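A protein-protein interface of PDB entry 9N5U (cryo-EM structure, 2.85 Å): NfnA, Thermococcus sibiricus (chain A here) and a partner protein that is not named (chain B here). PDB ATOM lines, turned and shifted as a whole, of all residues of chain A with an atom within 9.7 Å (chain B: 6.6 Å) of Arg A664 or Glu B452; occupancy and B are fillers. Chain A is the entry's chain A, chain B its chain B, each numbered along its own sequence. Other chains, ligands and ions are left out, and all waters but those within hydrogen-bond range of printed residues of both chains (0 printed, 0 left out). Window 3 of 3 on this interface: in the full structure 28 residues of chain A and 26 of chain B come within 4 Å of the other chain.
Of the 12 printed residues of chain A, 6 touch a printed residue of chain B.
Printed residues of chain A that touch a printed residue of chain B: Tyr A661, Leu A662, Phe A663, Arg A664, Gly A665 and Thr A668.
Hydrophobic or aromatic side chains of chain A that line the printed part of chain B: Tyr A661.
Along chain A the printed residues that touch a printed residue of chain B span positions 661 to 668.
Of the 17 printed residues of chain B, 6 touch a printed residue of chain A.
Among the printed residues, 12 pairs touch across the chains.
Among the printed residues, Asp or Glu carboxylates within 4 Å of a Lys or Arg side-chain nitrogen of the other chain: Arg A664 with Glu B452 (2.8 Å).
N of Leu A662 lies within hydrogen-bond range of O of Tyr A669.
O of Gly A665 lies within hydrogen-bond range of OG1 of Thr A668, at 2.8 Å.
OE1 of Glu B452 is in hydrogen-bond range of N of Phe B281.
The side-chain carboxylate (OD1) of Asp B447 is in salt-bridge range of the side-chain amino group (NZ) of Lys B451 (2.9 Å).
OG of Ser B453 is in hydrogen-bond range of N of Gly B455, at 3.2 Å.
Of the printed residues of chain B, Tyr A661 touches Arg B297 (3.5 Å).
Of the printed residues of chain B, Phe A663 touches Arg B297.
Of chain B, only Lys B451, Glu B452, Ser B453 and Cys B454 come within 4 Å of Arg A664.
Of the printed residues of chain B, Gly A665 touches Ser B453, Cys B454 and Gly B455.
Of the printed residues of chain B, Thr A668 touches Cys B454 (3.9 Å) and Gly B455 (3.9 Å).
No residue of chain A comes within 4 Å of Ala B280.
Printed residues of chain A within 4 Å of Lys B451: Arg A664.
Printed residues of chain A within 4 Å of Ser B453: Arg A664 and Gly A665.
The nearest printed residue of chain B that does not touch Tyr A661 is Gly B455 (4.6 Å).
Among the printed residues, pairs that only touch across the chains: Arg A664 with Ser B453, Gly A665 with Gly B455, Tyr A661 with Arg B297, Gly A665 with Cys B454, Arg A664 with Cys B454, Thr A668 with Cys B454, Thr A668 with Gly B455, Arg A664 with Lys B451 and Leu A662 with Arg B297.
NH1 of Arg A664 is in salt-bridge range of OE1 of Glu B452 (2.8 Å).
The backbone NH (N) of Gly A665 is in hydrogen-bond range of the backbone carbonyl oxygen (O) of Ser B453 (3.1 Å).
O of Phe A663 sits close to NH2 of Arg B297, at 2.3 Å.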
ATOM      1  N   ASN A 622      -6.891 -12.097 -10.817  1.00  0.00           N
ATOM      2  CA  ASN A 622      -7.059 -13.503 -10.482  1.00  0.00           C
ATOM      3  C   ASN A 622      -6.301 -13.796  -9.195  1.00  0.00           C
ATOM      4  O   ASN A 622      -5.098 -13.537  -9.105  1.00  0.00           O
ATOM      5  CB  ASN A 622      -6.558 -14.389 -11.617  1.00  0.00           C
ATOM      6  CG  ASN A 622      -7.584 -14.583 -12.705  1.00  0.00           C
ATOM      7  OD1 ASN A 622      -8.593 -15.255 -12.508  1.00  0.00           O
ATOM      8  ND2 ASN A 622      -7.325 -14.009 -13.868  1.00  0.00           N
ATOM      9  N   LEU A 642       1.603 -15.543 -18.358  1.00  0.00           N
ATOM     10  CA  LEU A 642       1.031 -16.446 -19.360  1.00  0.00           C
ATOM     11  C   LEU A 642       1.741 -16.296 -20.709  1.00  0.00           C
ATOM     12  O   LEU A 642       1.173 -15.849 -21.705  1.00  0.00           O
ATOM     13  CB  LEU A 642      -0.480 -16.231 -19.499  1.00  0.00           C
ATOM     14  CG  LEU A 642      -1.362 -16.914 -18.457  1.00  0.00           C
ATOM     15  CD1 LEU A 642      -2.808 -16.527 -18.662  1.00  0.00           C
ATOM     16  CD2 LEU A 642      -1.202 -18.415 -18.536  1.00  0.00           C
ATOM     17  N   TYR A 661      -1.780 -25.388 -19.744  1.00  0.00           N
ATOM     18  CA  TYR A 661      -2.828 -24.381 -19.693  1.00  0.00           C
ATOM     19  C   TYR A 661      -4.112 -24.986 -19.145  1.00  0.00           C
ATOM     20  O   TYR A 661      -4.524 -26.076 -19.547  1.00  0.00           O
ATOM     21  CB  TYR A 661      -3.097 -23.823 -21.089  1.00  0.00           C
ATOM     22  CG  TYR A 661      -2.123 -22.792 -21.604  1.00  0.00           C
ATOM     23  CD1 TYR A 661      -2.245 -21.461 -21.247  1.00  0.00           C
ATOM     24  CD2 TYR A 661      -1.118 -23.141 -22.493  1.00  0.00           C
ATOM     25  CE1 TYR A 661      -1.380 -20.511 -21.735  1.00  0.00           C
ATOM     26  CE2 TYR A 661      -0.245 -22.195 -22.986  1.00  0.00           C
ATOM     27  CZ  TYR A 661      -0.381 -20.881 -22.601  1.00  0.00           C
ATOM     28  OH  TYR A 661       0.477 -19.928 -23.085  1.00  0.00           O
ATOM     29  N   LEU A 662      -4.750 -24.274 -18.228  1.00  0.00           N
ATOM     30  CA  LEU A 662      -6.031 -24.693 -17.686  1.00  0.00           C
ATOM     31  C   LEU A 662      -7.040 -23.571 -17.866  1.00  0.00           C
ATOM     32  O   LEU A 662      -6.708 -22.396 -17.698  1.00  0.00           O
ATOM     33  CB  LEU A 662      -5.920 -25.075 -16.208  1.00  0.00           C
ATOM     34  CG  LEU A 662      -4.990 -26.239 -15.866  1.00  0.00           C
ATOM     35  CD1 LEU A 662      -4.903 -26.409 -14.366  1.00  0.00           C
ATOM     36  CD2 LEU A 662      -5.455 -27.525 -16.517  1.00  0.00           C
ATOM     37  N   PHE A 663      -8.265 -23.953 -18.236  1.00  0.00           N
ATOM     38  CA  PHE A 663      -9.405 -23.058 -18.413  1.00  0.00           C
ATOM     39  C   PHE A 663      -9.163 -22.029 -19.512  1.00  0.00           C
ATOM     40  O   PHE A 663      -8.156 -22.097 -20.221  1.00  0.00           O
ATOM     41  CB  PHE A 663      -9.768 -22.391 -17.086  1.00  0.00           C
ATOM     42  CG  PHE A 663     -10.207 -23.364 -16.032  1.00  0.00           C
ATOM     43  CD1 PHE A 663     -11.487 -23.885 -16.044  1.00  0.00           C
ATOM     44  CD2 PHE A 663      -9.335 -23.773 -15.041  1.00  0.00           C
ATOM     45  CE1 PHE A 663     -11.892 -24.787 -15.085  1.00  0.00           C
ATOM     46  CE2 PHE A 663      -9.734 -24.676 -14.081  1.00  0.00           C
ATOM     47  CZ  PHE A 663     -11.015 -25.183 -14.104  1.00  0.00           C
ATOM     48  N   ARG A 664     -10.084 -21.086 -19.678  1.00  0.00           N
ATOM     49  CA  ARG A 664     -10.109 -20.239 -20.860  1.00  0.00           C
ATOM     50  C   ARG A 664     -10.272 -18.774 -20.482  1.00  0.00           C
ATOM     51  O   ARG A 664     -10.915 -18.440 -19.485  1.00  0.00           O
ATOM     52  CB  ARG A 664     -11.250 -20.650 -21.793  1.00  0.00           C
ATOM     53  CG  ARG A 664     -10.946 -20.512 -23.260  1.00  0.00           C
ATOM     54  CD  ARG A 664     -12.217 -20.330 -24.061  1.00  0.00           C
ATOM     55  NE  ARG A 664     -13.286 -21.212 -23.616  1.00  0.00           N
ATOM     56  CZ  ARG A 664     -14.501 -21.235 -24.143  1.00  0.00           C
ATOM     57  NH1 ARG A 664     -14.837 -20.436 -25.140  1.00  0.00           N
ATOM     58  NH2 ARG A 664     -15.403 -22.081 -23.656  1.00  0.00           N
ATOM     59  N   GLY A 665      -9.690 -17.906 -21.298  1.00  0.00           N
ATOM     60  CA  GLY A 665      -9.980 -16.484 -21.199  1.00  0.00           C
ATOM     61  C   GLY A 665      -9.221 -15.817 -20.080  1.00  0.00           C
ATOM     62  O   GLY A 665      -8.004 -15.952 -19.969  1.00  0.00           O
ATOM     63  N   PHE A 666      -9.949 -15.068 -19.252  1.00  0.00           N
ATOM     64  CA  PHE A 666      -9.332 -14.387 -18.121  1.00  0.00           C
ATOM     65  C   PHE A 666      -8.964 -15.365 -17.015  1.00  0.00           C
ATOM     66  O   PHE A 666      -8.052 -15.093 -16.228  1.00  0.00           O
ATOM     67  CB  PHE A 666     -10.277 -13.310 -17.594  1.00  0.00           C
ATOM     68  CG  PHE A 666      -9.640 -12.364 -16.624  1.00  0.00           C
ATOM     69  CD1 PHE A 666      -8.643 -11.499 -17.035  1.00  0.00           C
ATOM     70  CD2 PHE A 666     -10.052 -12.324 -15.306  1.00  0.00           C
ATOM     71  CE1 PHE A 666      -8.061 -10.628 -16.150  1.00  0.00           C
ATOM     72  CE2 PHE A 666      -9.473 -11.451 -14.416  1.00  0.00           C
ATOM     73  CZ  PHE A 666      -8.479 -10.601 -14.839  1.00  0.00           C
ATOM     74  N   LYS A 667      -9.636 -16.511 -16.960  1.00  0.00           N
ATOM     75  CA  LYS A 667      -9.428 -17.492 -15.903  1.00  0.00           C
ATOM     76  C   LYS A 667      -8.282 -18.449 -16.195  1.00  0.00           C
ATOM     77  O   LYS A 667      -8.067 -19.382 -15.417  1.00  0.00           O
ATOM     78  CB  LYS A 667     -10.710 -18.293 -15.676  1.00  0.00           C
ATOM     79  CG  LYS A 667     -11.913 -17.452 -15.327  1.00  0.00           C
ATOM     80  CD  LYS A 667     -11.699 -16.700 -14.034  1.00  0.00           C
ATOM     81  CE  LYS A 667     -12.861 -15.779 -13.748  1.00  0.00           C
ATOM     82  NZ  LYS A 667     -12.619 -14.966 -12.532  1.00  0.00           N
ATOM     83  N   THR A 668      -7.553 -18.239 -17.286  1.00  0.00           N
ATOM     84  CA  THR A 668      -6.486 -19.147 -17.675  1.00  0.00           C
ATOM     85  C   THR A 668      -5.340 -19.101 -16.674  1.00  0.00           C
ATOM     86  O   THR A 668      -4.926 -18.029 -16.229  1.00  0.00           O
ATOM     87  CB  THR A 668      -5.975 -18.780 -19.069  1.00  0.00           C
ATOM     88  OG1 THR A 668      -7.085 -18.626 -19.958  1.00  0.00           O
ATOM     89  CG2 THR A 668      -5.050 -19.855 -19.607  1.00  0.00           C
ATOM     90  N   TYR A 669      -4.819 -20.273 -16.324  1.00  0.00           N
ATOM     91  CA  TYR A 669      -3.628 -20.341 -15.494  1.00  0.00           C
ATOM     92  C   TYR A 669      -2.858 -21.607 -15.840  1.00  0.00           C
ATOM     93  O   TYR A 669      -3.284 -22.417 -16.666  1.00  0.00           O
ATOM     94  CB  TYR A 669      -3.975 -20.266 -14.003  1.00  0.00           C
ATOM     95  CG  TYR A 669      -4.669 -21.472 -13.419  1.00  0.00           C
ATOM     96  CD1 TYR A 669      -6.041 -21.625 -13.523  1.00  0.00           C
ATOM     97  CD2 TYR A 669      -3.957 -22.437 -12.727  1.00  0.00           C
ATOM     98  CE1 TYR A 669      -6.676 -22.715 -12.978  1.00  0.00           C
ATOM     99  CE2 TYR A 669      -4.585 -23.529 -12.178  1.00  0.00           C
ATOM    100  CZ  TYR A 669      -5.944 -23.663 -12.306  1.00  0.00           C
ATOM    101  OH  TYR A 669      -6.570 -24.754 -11.758  1.00  0.00           O
ATOM    102  N   ILE A 670      -1.702 -21.755 -15.209  1.00  0.00           N
ATOM    103  CA  ILE A 670      -0.788 -22.859 -15.451  1.00  0.00           C
ATOM    104  C   ILE A 670      -0.783 -23.745 -14.216  1.00  0.00           C
ATOM    105  O   ILE A 670      -0.740 -23.250 -13.085  1.00  0.00           O
ATOM    106  CB  ILE A 670       0.630 -22.346 -15.773  1.00  0.00           C
ATOM    107  CG1 ILE A 670       0.588 -21.319 -16.908  1.00  0.00           C
ATOM    108  CG2 ILE A 670       1.547 -23.485 -16.132  1.00  0.00           C
ATOM    109  CD1 ILE A 670       0.325 -21.901 -18.265  1.00  0.00           C
ATOM    110  N   GLY B 197     -19.933 -19.919 -34.361  1.00  0.00           N
ATOM    111  CA  GLY B 197     -19.957 -19.500 -32.982  1.00  0.00           C
ATOM    112  C   GLY B 197     -20.680 -18.205 -32.728  1.00  0.00           C
ATOM    113  O   GLY B 197     -20.814 -17.798 -31.570  1.00  0.00           O
ATOM    114  N   ARG B 236     -20.557 -28.545 -34.773  1.00  0.00           N
ATOM    115  CA  ARG B 236     -20.619 -28.646 -33.324  1.00  0.00           C
ATOM    116  C   ARG B 236     -21.525 -29.792 -32.894  1.00  0.00           C
ATOM    117  O   ARG B 236     -22.476 -30.161 -33.587  1.00  0.00           O
ATOM    118  CB  ARG B 236     -21.116 -27.337 -32.714  1.00  0.00           C
ATOM    119  CG  ARG B 236     -20.159 -26.174 -32.866  1.00  0.00           C
ATOM    120  CD  ARG B 236     -20.853 -24.855 -32.585  1.00  0.00           C
ATOM    121  NE  ARG B 236     -20.603 -24.357 -31.238  1.00  0.00           N
ATOM    122  CZ  ARG B 236     -19.771 -23.366 -30.949  1.00  0.00           C
ATOM    123  NH1 ARG B 236     -19.076 -22.750 -31.890  1.00  0.00           N
ATOM    124  NH2 ARG B 236     -19.638 -22.979 -29.685  1.00  0.00           N
ATOM    125  N   GLY B 279     -17.279 -27.115 -28.920  1.00  0.00           N
ATOM    126  CA  GLY B 279     -18.014 -25.884 -28.717  1.00  0.00           C
ATOM    127  C   GLY B 279     -17.200 -24.746 -28.147  1.00  0.00           C
ATOM    128  O   GLY B 279     -17.037 -24.626 -26.930  1.00  0.00           O
ATOM    129  N   ALA B 280     -16.711 -23.882 -29.032  1.00  0.00           N
ATOM    130  CA  ALA B 280     -15.955 -22.699 -28.645  1.00  0.00           C
ATOM    131  C   ALA B 280     -15.961 -21.739 -29.822  1.00  0.00           C
ATOM    132  O   ALA B 280     -15.744 -22.158 -30.962  1.00  0.00           O
ATOM    133  CB  ALA B 280     -14.521 -23.054 -28.247  1.00  0.00           C
ATOM    134  N   PHE B 281     -16.211 -20.459 -29.541  1.00  0.00           N
ATOM    135  CA  PHE B 281     -16.249 -19.452 -30.597  1.00  0.00           C
ATOM    136  C   PHE B 281     -14.884 -19.262 -31.243  1.00  0.00           C
ATOM    137  O   PHE B 281     -14.801 -18.870 -32.411  1.00  0.00           O
ATOM    138  CB  PHE B 281     -16.764 -18.132 -30.024  1.00  0.00           C
ATOM    139  CG  PHE B 281     -16.815 -17.007 -31.016  1.00  0.00           C
ATOM    140  CD1 PHE B 281     -17.784 -16.978 -31.993  1.00  0.00           C
ATOM    141  CD2 PHE B 281     -15.914 -15.966 -30.954  1.00  0.00           C
ATOM    142  CE1 PHE B 281     -17.848 -15.947 -32.899  1.00  0.00           C
ATOM    143  CE2 PHE B 281     -15.977 -14.931 -31.859  1.00  0.00           C
ATOM    144  CZ  PHE B 281     -16.941 -14.924 -32.833  1.00  0.00           C
ATOM    145  N   VAL B 282     -13.809 -19.532 -30.503  1.00  0.00           N
ATOM    146  CA  VAL B 282     -12.470 -19.375 -31.054  1.00  0.00           C
ATOM    147  C   VAL B 282     -12.096 -20.536 -31.965  1.00  0.00           C
ATOM    148  O   VAL B 282     -11.226 -20.382 -32.826  1.00  0.00           O
ATOM    149  CB  VAL B 282     -11.455 -19.203 -29.910  1.00  0.00           C
ATOM    150  CG1 VAL B 282     -11.289 -20.495 -29.137  1.00  0.00           C
ATOM    151  CG2 VAL B 282     -10.119 -18.696 -30.431  1.00  0.00           C
ATOM    152  N   ARG B 297      -5.842 -27.819 -27.494  1.00  0.00           N
ATOM    153  CA  ARG B 297      -6.687 -26.679 -27.178  1.00  0.00           C
ATOM    154  C   ARG B 297      -6.842 -25.785 -28.401  1.00  0.00           C
ATOM    155  O   ARG B 297      -5.926 -25.640 -29.214  1.00  0.00           O
ATOM    156  CB  ARG B 297      -6.099 -25.869 -26.025  1.00  0.00           C
ATOM    157  CG  ARG B 297      -5.892 -26.650 -24.759  1.00  0.00           C
ATOM    158  CD  ARG B 297      -5.168 -25.825 -23.714  1.00  0.00           C
ATOM    159  NE  ARG B 297      -6.083 -25.139 -22.812  1.00  0.00           N
ATOM    160  CZ  ARG B 297      -6.205 -23.823 -22.724  1.00  0.00           C
ATOM    161  NH1 ARG B 297      -5.487 -23.010 -23.478  1.00  0.00           N
ATOM    162  NH2 ARG B 297      -7.062 -23.309 -21.850  1.00  0.00           N
ATOM    163  N   ASP B 447     -18.918  -8.781 -23.193  1.00  0.00           N
ATOM    164  CA  ASP B 447     -19.074  -9.892 -22.261  1.00  0.00           C
ATOM    165  C   ASP B 447     -18.898 -11.225 -22.974  1.00  0.00           C
ATOM    166  O   ASP B 447     -18.189 -12.120 -22.490  1.00  0.00           O
ATOM    167  CB  ASP B 447     -20.451  -9.801 -21.602  1.00  0.00           C
ATOM    168  CG  ASP B 447     -20.693 -10.887 -20.584  1.00  0.00           C
ATOM    169  OD1 ASP B 447     -19.714 -11.475 -20.081  1.00  0.00           O
ATOM    170  OD2 ASP B 447     -21.875 -11.154 -20.286  1.00  0.00           O
ATOM    171  N   PHE B 448     -19.527 -11.366 -24.142  1.00  0.00           N
ATOM    172  CA  PHE B 448     -19.352 -12.583 -24.925  1.00  0.00           C
ATOM    173  C   PHE B 448     -17.898 -12.761 -25.343  1.00  0.00           C
ATOM    174  O   PHE B 448     -17.356 -13.869 -25.269  1.00  0.00           O
ATOM    175  CB  PHE B 448     -20.270 -12.558 -26.146  1.00  0.00           C
ATOM    176  CG  PHE B 448     -20.184 -13.791 -26.991  1.00  0.00           C
ATOM    177  CD1 PHE B 448     -20.781 -14.968 -26.583  1.00  0.00           C
ATOM    178  CD2 PHE B 448     -19.510 -13.774 -28.196  1.00  0.00           C
ATOM    179  CE1 PHE B 448     -20.701 -16.102 -27.359  1.00  0.00           C
ATOM    180  CE2 PHE B 448     -19.431 -14.904 -28.974  1.00  0.00           C
ATOM    181  CZ  PHE B 448     -20.027 -16.069 -28.554  1.00  0.00           C
ATOM    182  N   THR B 449     -17.247 -11.674 -25.765  1.00  0.00           N
ATOM    183  CA  THR B 449     -15.842 -11.756 -26.157  1.00  0.00           C
ATOM    184  C   THR B 449     -14.952 -12.160 -24.985  1.00  0.00           C
ATOM    185  O   THR B 449     -14.018 -12.952 -25.151  1.00  0.00           O
ATOM    186  CB  THR B 449     -15.385 -10.420 -26.735  1.00  0.00           C
ATOM    187  OG1 THR B 449     -16.145 -10.118 -27.912  1.00  0.00           O
ATOM    188  CG2 THR B 449     -13.925 -10.488 -27.090  1.00  0.00           C
ATOM    189  N   VAL B 450     -15.227 -11.621 -23.794  1.00  0.00           N
ATOM    190  CA  VAL B 450     -14.463 -11.978 -22.602  1.00  0.00           C
ATOM    191  C   VAL B 450     -14.628 -13.459 -22.288  1.00  0.00           C
ATOM    192  O   VAL B 450     -13.656 -14.148 -21.952  1.00  0.00           O
ATOM    193  CB  VAL B 450     -14.882 -11.089 -21.413  1.00  0.00           C
ATOM    194  CG1 VAL B 450     -14.432 -11.686 -20.094  1.00  0.00           C
ATOM    195  CG2 VAL B 450     -14.304  -9.704 -21.565  1.00  0.00           C
ATOM    196  N   LYS B 451     -15.856 -13.973 -22.398  1.00  0.00           N
ATOM    197  CA  LYS B 451     -16.089 -15.395 -22.153  1.00  0.00           C
ATOM    198  C   LYS B 451     -15.364 -16.274 -23.167  1.00  0.00           C
ATOM    199  O   LYS B 451     -14.776 -17.298 -22.803  1.00  0.00           O
ATOM    200  CB  LYS B 451     -17.586 -15.696 -22.183  1.00  0.00           C
ATOM    201  CG  LYS B 451     -18.218 -15.961 -20.835  1.00  0.00           C
ATOM    202  CD  LYS B 451     -18.647 -14.682 -20.160  1.00  0.00           C
ATOM    203  CE  LYS B 451     -19.538 -14.969 -18.971  1.00  0.00           C
ATOM    204  NZ  LYS B 451     -19.949 -13.720 -18.276  1.00  0.00           N
ATOM    205  N   GLU B 452     -15.397 -15.893 -24.443  1.00  0.00           N
ATOM    206  CA  GLU B 452     -14.977 -16.780 -25.521  1.00  0.00           C
ATOM    207  C   GLU B 452     -13.506 -16.660 -25.886  1.00  0.00           C
ATOM    208  O   GLU B 452     -13.033 -17.437 -26.721  1.00  0.00           O
ATOM    209  CB  GLU B 452     -15.821 -16.521 -26.770  1.00  0.00           C
ATOM    210  CG  GLU B 452     -17.278 -16.867 -26.592  1.00  0.00           C
ATOM    211  CD  GLU B 452     -17.506 -18.350 -26.385  1.00  0.00           C
ATOM    212  OE1 GLU B 452     -16.688 -19.157 -26.874  1.00  0.00           O
ATOM    213  OE2 GLU B 452     -18.506 -18.712 -25.731  1.00  0.00           O
ATOM    214  N   SER B 453     -12.781 -15.717 -25.298  1.00  0.00           N
ATOM    215  CA  SER B 453     -11.359 -15.587 -25.577  1.00  0.00           C
ATOM    216  C   SER B 453     -10.611 -16.820 -25.091  1.00  0.00           C
ATOM    217  O   SER B 453     -10.947 -17.398 -24.056  1.00  0.00           O
ATOM    218  CB  SER B 453     -10.807 -14.331 -24.907  1.00  0.00           C
ATOM    219  OG  SER B 453      -9.395 -14.309 -24.955  1.00  0.00           O
ATOM    220  N   CYS B 454      -9.599 -17.234 -25.849  1.00  0.00           N
ATOM    221  CA  CYS B 454      -8.808 -18.388 -25.446  1.00  0.00           C
ATOM    222  C   CYS B 454      -7.780 -18.056 -24.374  1.00  0.00           C
ATOM    223  O   CYS B 454      -7.196 -18.978 -23.794  1.00  0.00           O
ATOM    224  CB  CYS B 454      -8.106 -19.007 -26.657  1.00  0.00           C
ATOM    225  SG  CYS B 454      -6.735 -18.056 -27.327  1.00  0.00           S
ATOM    226  N   GLY B 455      -7.553 -16.780 -24.088  1.00  0.00           N
ATOM    227  CA  GLY B 455      -6.588 -16.397 -23.076  1.00  0.00           C
ATOM    228  C   GLY B 455      -5.150 -16.718 -23.416  1.00  0.00           C
ATOM    229  O   GLY B 455      -4.399 -17.172 -22.545  1.00  0.00           O
ATOM    230  N   LEU B 502     -10.556 -12.869 -33.259  1.00  0.00           N
ATOM    231  CA  LEU B 502     -11.515 -12.622 -32.185  1.00  0.00           C
ATOM    232  C   LEU B 502     -11.172 -11.346 -31.431  1.00  0.00           C
ATOM    233  O   LEU B 502     -12.054 -10.527 -31.157  1.00  0.00           O
ATOM    234  CB  LEU B 502     -11.576 -13.816 -31.231  1.00  0.00           C
ATOM    235  CG  LEU B 502     -12.317 -13.680 -29.892  1.00  0.00           C
ATOM    236  CD1 LEU B 502     -13.694 -13.072 -30.047  1.00  0.00           C
ATOM    237  CD2 LEU B 502     -12.433 -15.030 -29.220  1.00  0.00           C
